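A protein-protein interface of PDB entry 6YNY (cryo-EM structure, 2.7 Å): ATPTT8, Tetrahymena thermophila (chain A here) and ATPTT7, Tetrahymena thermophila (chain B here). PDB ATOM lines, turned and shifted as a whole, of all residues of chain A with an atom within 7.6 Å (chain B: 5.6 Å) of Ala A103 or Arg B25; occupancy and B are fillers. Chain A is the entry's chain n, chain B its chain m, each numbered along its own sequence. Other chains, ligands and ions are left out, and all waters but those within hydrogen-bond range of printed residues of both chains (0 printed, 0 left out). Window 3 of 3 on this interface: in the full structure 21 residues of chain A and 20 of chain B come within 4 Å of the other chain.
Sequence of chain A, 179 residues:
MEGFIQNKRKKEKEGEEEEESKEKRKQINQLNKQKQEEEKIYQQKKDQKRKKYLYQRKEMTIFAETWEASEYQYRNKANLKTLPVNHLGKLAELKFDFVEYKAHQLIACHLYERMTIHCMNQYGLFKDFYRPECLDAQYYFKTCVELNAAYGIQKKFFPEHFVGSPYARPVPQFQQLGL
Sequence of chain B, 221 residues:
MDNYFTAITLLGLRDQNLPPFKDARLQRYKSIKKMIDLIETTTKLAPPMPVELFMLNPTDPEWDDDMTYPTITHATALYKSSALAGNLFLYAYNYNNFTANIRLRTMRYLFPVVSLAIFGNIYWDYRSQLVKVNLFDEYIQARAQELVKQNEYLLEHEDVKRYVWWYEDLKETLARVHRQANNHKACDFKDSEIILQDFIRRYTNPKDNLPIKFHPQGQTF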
ATOM      1  N   PHE A  63     -10.895  11.173  -4.983  1.00  0.00           N
ATOM      2  CA  PHE A  63     -12.052  10.309  -5.174  1.00  0.00           C
ATOM      3  C   PHE A  63     -12.254   9.378  -3.985  1.00  0.00           C
ATOM      4  O   PHE A  63     -12.598   8.206  -4.142  1.00  0.00           O
ATOM      5  CB  PHE A  63     -11.916   9.518  -6.468  1.00  0.00           C
ATOM      6  CG  PHE A  63     -11.874  10.380  -7.693  1.00  0.00           C
ATOM      7  CD1 PHE A  63     -13.018  11.001  -8.154  1.00  0.00           C
ATOM      8  CD2 PHE A  63     -10.695  10.577  -8.382  1.00  0.00           C
ATOM      9  CE1 PHE A  63     -12.987  11.795  -9.273  1.00  0.00           C
ATOM     10  CE2 PHE A  63     -10.663  11.374  -9.506  1.00  0.00           C
ATOM     11  CZ  PHE A  63     -11.809  11.982  -9.948  1.00  0.00           C
ATOM     12  N   ALA A  64     -12.025   9.888  -2.781  1.00  0.00           N
ATOM     13  CA  ALA A  64     -12.199   9.106  -1.567  1.00  0.00           C
ATOM     14  C   ALA A  64     -12.398  10.064  -0.402  1.00  0.00           C
ATOM     15  O   ALA A  64     -12.357  11.286  -0.562  1.00  0.00           O
ATOM     16  CB  ALA A  64     -11.003   8.185  -1.330  1.00  0.00           C
ATOM     17  N   GLU A  65     -12.623   9.493   0.779  1.00  0.00           N
ATOM     18  CA  GLU A  65     -12.744  10.278   1.997  1.00  0.00           C
ATOM     19  C   GLU A  65     -11.405  10.510   2.675  1.00  0.00           C
ATOM     20  O   GLU A  65     -11.278  11.453   3.465  1.00  0.00           O
ATOM     21  CB  GLU A  65     -13.666   9.581   2.998  1.00  0.00           C
ATOM     22  CG  GLU A  65     -14.932   9.017   2.418  1.00  0.00           C
ATOM     23  CD  GLU A  65     -15.838   8.436   3.481  1.00  0.00           C
ATOM     24  OE1 GLU A  65     -16.230   9.180   4.403  1.00  0.00           O
ATOM     25  OE2 GLU A  65     -16.150   7.230   3.405  1.00  0.00           O
ATOM     26  N   GLU A 100     -26.755  15.663  11.580  1.00  0.00           N
ATOM     27  CA  GLU A 100     -25.605  15.450  10.717  1.00  0.00           C
ATOM     28  C   GLU A 100     -25.288  13.968  10.670  1.00  0.00           C
ATOM     29  O   GLU A 100     -25.250  13.304  11.710  1.00  0.00           O
ATOM     30  CB  GLU A 100     -24.387  16.237  11.206  1.00  0.00           C
ATOM     31  CG  GLU A 100     -24.208  17.575  10.518  1.00  0.00           C
ATOM     32  CD  GLU A 100     -23.909  17.435   9.040  1.00  0.00           C
ATOM     33  OE1 GLU A 100     -23.605  16.308   8.596  1.00  0.00           O
ATOM     34  OE2 GLU A 100     -23.984  18.450   8.318  1.00  0.00           O
ATOM     35  N   TYR A 101     -25.063  13.457   9.466  1.00  0.00           N
ATOM     36  CA  TYR A 101     -24.717  12.060   9.278  1.00  0.00           C
ATOM     37  C   TYR A 101     -23.205  11.907   9.213  1.00  0.00           C
ATOM     38  O   TYR A 101     -22.509  12.716   8.595  1.00  0.00           O
ATOM     39  CB  TYR A 101     -25.354  11.514   8.001  1.00  0.00           C
ATOM     40  CG  TYR A 101     -26.861  11.586   7.985  1.00  0.00           C
ATOM     41  CD1 TYR A 101     -27.621  10.782   8.815  1.00  0.00           C
ATOM     42  CD2 TYR A 101     -27.525  12.450   7.130  1.00  0.00           C
ATOM     43  CE1 TYR A 101     -28.993  10.842   8.802  1.00  0.00           C
ATOM     44  CE2 TYR A 101     -28.898  12.514   7.110  1.00  0.00           C
ATOM     45  CZ  TYR A 101     -29.627  11.706   7.947  1.00  0.00           C
ATOM     46  OH  TYR A 101     -30.999  11.765   7.934  1.00  0.00           O
ATOM     47  N   LYS A 102     -22.702  10.857   9.861  1.00  0.00           N
ATOM     48  CA  LYS A 102     -21.268  10.608   9.882  1.00  0.00           C
ATOM     49  C   LYS A 102     -20.717  10.281   8.504  1.00  0.00           C
ATOM     50  O   LYS A 102     -19.499  10.341   8.308  1.00  0.00           O
ATOM     51  CB  LYS A 102     -20.954   9.464  10.841  1.00  0.00           C
ATOM     52  CG  LYS A 102     -21.466   9.672  12.248  1.00  0.00           C
ATOM     53  CD  LYS A 102     -20.756  10.807  12.935  1.00  0.00           C
ATOM     54  CE  LYS A 102     -21.137  10.878  14.397  1.00  0.00           C
ATOM     55  NZ  LYS A 102     -20.390  11.937  15.114  1.00  0.00           N
ATOM     56  N   ALA A 103     -21.575   9.936   7.550  1.00  0.00           N
ATOM     57  CA  ALA A 103     -21.130   9.556   6.218  1.00  0.00           C
ATOM     58  C   ALA A 103     -20.730  10.745   5.359  1.00  0.00           C
ATOM     59  O   ALA A 103     -20.380  10.550   4.191  1.00  0.00           O
ATOM     60  CB  ALA A 103     -22.232   8.766   5.516  1.00  0.00           C
ATOM     61  N   HIS A 104     -20.775  11.959   5.899  1.00  0.00           N
ATOM     62  CA  HIS A 104     -20.481  13.163   5.140  1.00  0.00           C
ATOM     63  C   HIS A 104     -19.373  14.002   5.755  1.00  0.00           C
ATOM     64  O   HIS A 104     -19.048  15.062   5.209  1.00  0.00           O
ATOM     65  CB  HIS A 104     -21.743  14.025   5.011  1.00  0.00           C
ATOM     66  CG  HIS A 104     -22.905  13.316   4.393  1.00  0.00           C
ATOM     67  ND1 HIS A 104     -24.207  13.715   4.596  1.00  0.00           N
ATOM     68  CD2 HIS A 104     -22.964  12.241   3.573  1.00  0.00           C
ATOM     69  CE1 HIS A 104     -25.019  12.913   3.931  1.00  0.00           C
ATOM     70  NE2 HIS A 104     -24.289  12.010   3.303  1.00  0.00           N
ATOM     71  N   GLN A 105     -18.779  13.564   6.862  1.00  0.00           N
ATOM     72  CA  GLN A 105     -17.857  14.405   7.609  1.00  0.00           C
ATOM     73  C   GLN A 105     -16.408  14.251   7.178  1.00  0.00           C
ATOM     74  O   GLN A 105     -15.602  15.151   7.442  1.00  0.00           O
ATOM     75  CB  GLN A 105     -17.965  14.100   9.105  1.00  0.00           C
ATOM     76  CG  GLN A 105     -17.499  12.717   9.488  1.00  0.00           C
ATOM     77  CD  GLN A 105     -17.690  12.422  10.955  1.00  0.00           C
ATOM     78  OE1 GLN A 105     -18.370  13.160  11.666  1.00  0.00           O
ATOM     79  NE2 GLN A 105     -17.082  11.341  11.422  1.00  0.00           N
ATOM     80  N   LEU A 106     -16.055  13.150   6.522  1.00  0.00           N
ATOM     81  CA  LEU A 106     -14.668  12.916   6.144  1.00  0.00           C
ATOM     82  C   LEU A 106     -14.304  13.517   4.797  1.00  0.00           C
ATOM     83  O   LEU A 106     -13.157  13.937   4.610  1.00  0.00           O
ATOM     84  CB  LEU A 106     -14.376  11.417   6.113  1.00  0.00           C
ATOM     85  CG  LEU A 106     -14.493  10.687   7.445  1.00  0.00           C
ATOM     86  CD1 LEU A 106     -14.106   9.239   7.277  1.00  0.00           C
ATOM     87  CD2 LEU A 106     -13.639  11.351   8.501  1.00  0.00           C
ATOM     88  N   ILE A 107     -15.244  13.568   3.854  1.00  0.00           N
ATOM     89  CA  ILE A 107     -14.936  14.144   2.558  1.00  0.00           C
ATOM     90  C   ILE A 107     -14.479  15.589   2.733  1.00  0.00           C
ATOM     91  O   ILE A 107     -14.956  16.320   3.610  1.00  0.00           O
ATOM     92  CB  ILE A 107     -16.143  14.046   1.612  1.00  0.00           C
ATOM     93  CG1 ILE A 107     -15.853  14.782   0.309  1.00  0.00           C
ATOM     94  CG2 ILE A 107     -17.388  14.587   2.274  1.00  0.00           C
ATOM     95  CD1 ILE A 107     -16.756  14.381  -0.812  1.00  0.00           C
ATOM     96  N   HIS A 110     -16.445  19.529   2.945  1.00  0.00           N
ATOM     97  CA  HIS A 110     -17.902  19.477   2.921  1.00  0.00           C
ATOM     98  C   HIS A 110     -18.501  19.692   4.303  1.00  0.00           C
ATOM     99  O   HIS A 110     -19.537  20.353   4.435  1.00  0.00           O
ATOM    100  CB  HIS A 110     -18.363  18.140   2.347  1.00  0.00           C
ATOM    101  CG  HIS A 110     -19.832  18.073   2.079  1.00  0.00           C
ATOM    102  ND1 HIS A 110     -20.482  18.974   1.265  1.00  0.00           N
ATOM    103  CD2 HIS A 110     -20.779  17.213   2.519  1.00  0.00           C
ATOM    104  CE1 HIS A 110     -21.766  18.671   1.215  1.00  0.00           C
ATOM    105  NE2 HIS A 110     -21.972  17.608   1.968  1.00  0.00           N
ATOM    106  N   LEU B  18     -25.448  10.368   0.890  1.00  0.00           N
ATOM    107  CA  LEU B  18     -24.681   9.212   0.476  1.00  0.00           C
ATOM    108  C   LEU B  18     -25.082   7.985   1.286  1.00  0.00           C
ATOM    109  O   LEU B  18     -25.600   8.104   2.398  1.00  0.00           O
ATOM    110  CB  LEU B  18     -23.191   9.477   0.656  1.00  0.00           C
ATOM    111  CG  LEU B  18     -22.657  10.753   0.017  1.00  0.00           C
ATOM    112  CD1 LEU B  18     -21.234  11.001   0.457  1.00  0.00           C
ATOM    113  CD2 LEU B  18     -22.735  10.659  -1.484  1.00  0.00           C
ATOM    114  N   PRO B  19     -24.852   6.792   0.748  1.00  0.00           N
ATOM    115  CA  PRO B  19     -25.137   5.578   1.503  1.00  0.00           C
ATOM    116  C   PRO B  19     -24.268   5.501   2.743  1.00  0.00           C
ATOM    117  O   PRO B  19     -23.091   5.892   2.711  1.00  0.00           O
ATOM    118  CB  PRO B  19     -24.806   4.456   0.509  1.00  0.00           C
ATOM    119  CG  PRO B  19     -23.921   5.079  -0.496  1.00  0.00           C
ATOM    120  CD  PRO B  19     -24.360   6.491  -0.605  1.00  0.00           C
ATOM    121  N   PRO B  20     -24.802   5.003   3.858  1.00  0.00           N
ATOM    122  CA  PRO B  20     -24.053   5.009   5.117  1.00  0.00           C
ATOM    123  C   PRO B  20     -23.000   3.920   5.243  1.00  0.00           C
ATOM    124  O   PRO B  20     -22.458   3.740   6.335  1.00  0.00           O
ATOM    125  CB  PRO B  20     -25.162   4.813   6.159  1.00  0.00           C
ATOM    126  CG  PRO B  20     -26.186   4.026   5.460  1.00  0.00           C
ATOM    127  CD  PRO B  20     -26.152   4.442   4.026  1.00  0.00           C
ATOM    128  N   PHE B  21     -22.695   3.195   4.172  1.00  0.00           N
ATOM    129  CA  PHE B  21     -21.723   2.112   4.202  1.00  0.00           C
ATOM    130  C   PHE B  21     -20.585   2.417   3.241  1.00  0.00           C
ATOM    131  O   PHE B  21     -20.805   2.944   2.147  1.00  0.00           O
ATOM    132  CB  PHE B  21     -22.388   0.786   3.861  1.00  0.00           C
ATOM    133  CG  PHE B  21     -23.528   0.446   4.770  1.00  0.00           C
ATOM    134  CD1 PHE B  21     -23.294  -0.040   6.041  1.00  0.00           C
ATOM    135  CD2 PHE B  21     -24.833   0.629   4.362  1.00  0.00           C
ATOM    136  CE1 PHE B  21     -24.338  -0.342   6.880  1.00  0.00           C
ATOM    137  CE2 PHE B  21     -25.878   0.326   5.198  1.00  0.00           C
ATOM    138  CZ  PHE B  21     -25.632  -0.157   6.456  1.00  0.00           C
ATOM    139  N   LYS B  22     -19.365   2.071   3.658  1.00  0.00           N
ATOM    140  CA  LYS B  22     -18.181   2.460   2.900  1.00  0.00           C
ATOM    141  C   LYS B  22     -18.142   1.807   1.526  1.00  0.00           C
ATOM    142  O   LYS B  22     -17.703   2.430   0.551  1.00  0.00           O
ATOM    143  CB  LYS B  22     -16.919   2.095   3.677  1.00  0.00           C
ATOM    144  CG  LYS B  22     -16.619   2.975   4.861  1.00  0.00           C
ATOM    145  CD  LYS B  22     -15.387   2.473   5.576  1.00  0.00           C
ATOM    146  CE  LYS B  22     -14.941   3.407   6.673  1.00  0.00           C
ATOM    147  NZ  LYS B  22     -13.853   2.797   7.483  1.00  0.00           N
ATOM    148  N   ASP B  23     -18.590   0.558   1.421  1.00  0.00           N
ATOM    149  CA  ASP B  23     -18.483  -0.156   0.152  1.00  0.00           C
ATOM    150  C   ASP B  23     -19.164   0.618  -0.969  1.00  0.00           C
ATOM    151  O   ASP B  23     -18.535   0.965  -1.974  1.00  0.00           O
ATOM    152  CB  ASP B  23     -19.083  -1.553   0.289  1.00  0.00           C
ATOM    153  CG  ASP B  23     -18.758  -2.441  -0.890  1.00  0.00           C
ATOM    154  OD1 ASP B  23     -17.998  -2.002  -1.776  1.00  0.00           O
ATOM    155  OD2 ASP B  23     -19.263  -3.582  -0.931  1.00  0.00           O
ATOM    156  N   ALA B  24     -20.453   0.911  -0.807  1.00  0.00           N
ATOM    157  CA  ALA B  24     -21.172   1.642  -1.841  1.00  0.00           C
ATOM    158  C   ALA B  24     -20.769   3.108  -1.881  1.00  0.00           C
ATOM    159  O   ALA B  24     -20.841   3.741  -2.940  1.00  0.00           O
ATOM    160  CB  ALA B  24     -22.673   1.520  -1.614  1.00  0.00           C
ATOM    161  N   ARG B  25     -20.346   3.662  -0.748  1.00  0.00           N
ATOM    162  CA  ARG B  25     -19.989   5.074  -0.704  1.00  0.00           C
ATOM    163  C   ARG B  25     -18.697   5.337  -1.465  1.00  0.00           C
ATOM    164  O   ARG B  25     -18.566   6.361  -2.144  1.00  0.00           O
ATOM    165  CB  ARG B  25     -19.864   5.523   0.746  1.00  0.00           C
ATOM    166  CG  ARG B  25     -19.844   7.015   0.956  1.00  0.00           C
ATOM    167  CD  ARG B  25     -19.300   7.330   2.324  1.00  0.00           C
ATOM    168  NE  ARG B  25     -19.996   6.582   3.362  1.00  0.00           N
ATOM    169  CZ  ARG B  25     -19.488   6.310   4.558  1.00  0.00           C
ATOM    170  NH1 ARG B  25     -18.272   6.715   4.874  1.00  0.00           N
ATOM    171  NH2 ARG B  25     -20.196   5.622   5.436  1.00  0.00           N
ATOM    172  N   LEU B  26     -17.733   4.423  -1.365  1.00  0.00           N
ATOM    173  CA  LEU B  26     -16.465   4.595  -2.060  1.00  0.00           C
ATOM    174  C   LEU B  26     -16.582   4.290  -3.547  1.00  0.00           C
ATOM    175  O   LEU B  26     -15.838   4.863  -4.349  1.00  0.00           O
ATOM    176  CB  LEU B  26     -15.395   3.710  -1.424  1.00  0.00           C
ATOM    177  CG  LEU B  26     -14.611   4.317  -0.256  1.00  0.00           C
ATOM    178  CD1 LEU B  26     -15.521   4.779   0.864  1.00  0.00           C
ATOM    179  CD2 LEU B  26     -13.600   3.319   0.270  1.00  0.00           C
ATOM    180  N   GLN B  27     -17.490   3.394  -3.934  1.00  0.00           N
ATOM    181  CA  GLN B  27     -17.732   3.166  -5.352  1.00  0.00           C
ATOM    182  C   GLN B  27     -18.343   4.392  -6.010  1.00  0.00           C
ATOM    183  O   GLN B  27     -18.075   4.667  -7.184  1.00  0.00           O
ATOM    184  CB  GLN B  27     -18.657   1.969  -5.545  1.00  0.00           C
ATOM    185  CG  GLN B  27     -18.088   0.655  -5.107  1.00  0.00           C
ATOM    186  CD  GLN B  27     -19.127  -0.440  -5.116  1.00  0.00           C
ATOM    187  OE1 GLN B  27     -20.114  -0.365  -5.844  1.00  0.00           O
ATOM    188  NE2 GLN B  27     -18.919  -1.462  -4.296  1.00  0.00           N
ATOM    189  N   ARG B  28     -19.166   5.132  -5.269  1.00  0.00           N
ATOM    190  CA  ARG B  28     -19.803   6.319  -5.817  1.00  0.00           C
ATOM    191  C   ARG B  28     -18.800   7.443  -6.031  1.00  0.00           C
ATOM    192  O   ARG B  28     -18.988   8.279  -6.921  1.00  0.00           O
ATOM    193  CB  ARG B  28     -20.923   6.763  -4.885  1.00  0.00           C
ATOM    194  CG  ARG B  28     -21.846   7.811  -5.450  1.00  0.00           C
ATOM    195  CD  ARG B  28     -22.899   8.166  -4.434  1.00  0.00           C
ATOM    196  NE  ARG B  28     -23.898   9.092  -4.954  1.00  0.00           N
ATOM    197  CZ  ARG B  28     -24.985   8.722  -5.622  1.00  0.00           C
ATOM    198  NH1 ARG B  28     -25.221   7.444  -5.869  1.00  0.00           N
ATOM    199  NH2 ARG B  28     -25.839   9.636  -6.047  1.00  0.00           N
ATOM    200  N   TYR B  29     -17.735   7.482  -5.229  1.00  0.00           N
ATOM    201  CA  TYR B  29     -16.687   8.474  -5.444  1.00  0.00           C
ATOM    202  C   TYR B  29     -15.933   8.198  -6.736  1.00  0.00           C
ATOM    203  O   TYR B  29     -15.629   9.124  -7.495  1.00  0.00           O
ATOM    204  CB  TYR B  29     -15.720   8.482  -4.265  1.00  0.00           C
ATOM    205  CG  TYR B  29     -16.319   8.899  -2.946  1.00  0.00           C
ATOM    206  CD1 TYR B  29     -17.329   9.840  -2.883  1.00  0.00           C
ATOM    207  CD2 TYR B  29     -15.861   8.355  -1.759  1.00  0.00           C
ATOM    208  CE1 TYR B  29     -17.870  10.223  -1.677  1.00  0.00           C
ATOM    209  CE2 TYR B  29     -16.395   8.730  -0.552  1.00  0.00           C
ATOM    210  CZ  TYR B  29     -17.398   9.665  -0.515  1.00  0.00           C
ATOM    211  OH  TYR B  29     -17.931  10.041   0.694  1.00  0.00           O
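Printed residues of chain A that touch a printed residue of chain B: Phe A63, Ala A64, Glu A65, Ala A103 and His A104. Hydrophobic or aromatic side chains of chain A that line the printed part of chain B: Phe A63, Ala A103 and His A104. Of the 12 printed residues of chain B, 4 touch a printed residue of chain A. Hydrophobic or aromatic side chains of chain B within 4 Å of the printed part of chain A: Leu B18, Leu B26 and Tyr B29. Among the printed residues, 8 pairs touch across the chains.
Tyr B29 touches Phe A63. CA of Ala A64 touches CD2 of Tyr B29, at 3.7 Å. Glu A65 touches Leu B26. Glu A65 touches Tyr B29 (CG to CE2, 3.3 Å). Ala A103 touches Leu B18. NH2 of Arg B25 touches CB of Ala A103, at 3.7 Å.
NE2 of His A104 is in hydrogen-bond range of N of Leu B18, 3.1 Å away. The guanidinium group (NH1) of Arg B25 is in salt-bridge range of the side-chain carboxylate (OE2) of Glu A65 (2.6 Å).
Of chain B, only Leu B18 and Arg B25 come within 4 Å of Ala A103. Of chain A, only Glu A65 and Ala A103 come within 4 Å of Arg B25. Of the printed residues of chain B, His A104 touches Leu B18. Printed residues of chain B within 4 Å of Ala A64: Tyr B29 (3.7 Å). Printed residues of chain A within 4 Å of Leu B18: Ala A103 and His A104. Printed residues of chain A within 4 Å of Leu B26: Glu A65 (3.6 Å). His A110 touches none of the printed residues of chain B. Pro B20 touches none of the printed residues of chain A. The nearest residue of chain B that does not touch Ala A103 is Pro B19 (4.1 Å).
The guanidinium group of Arg B25 sits at hydrogen-bond distance from the backbone carbonyl oxygen of Pro B20. O of Pro B19 sits at hydrogen-bond distance from NE of Arg B25, 3.2 Å away.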
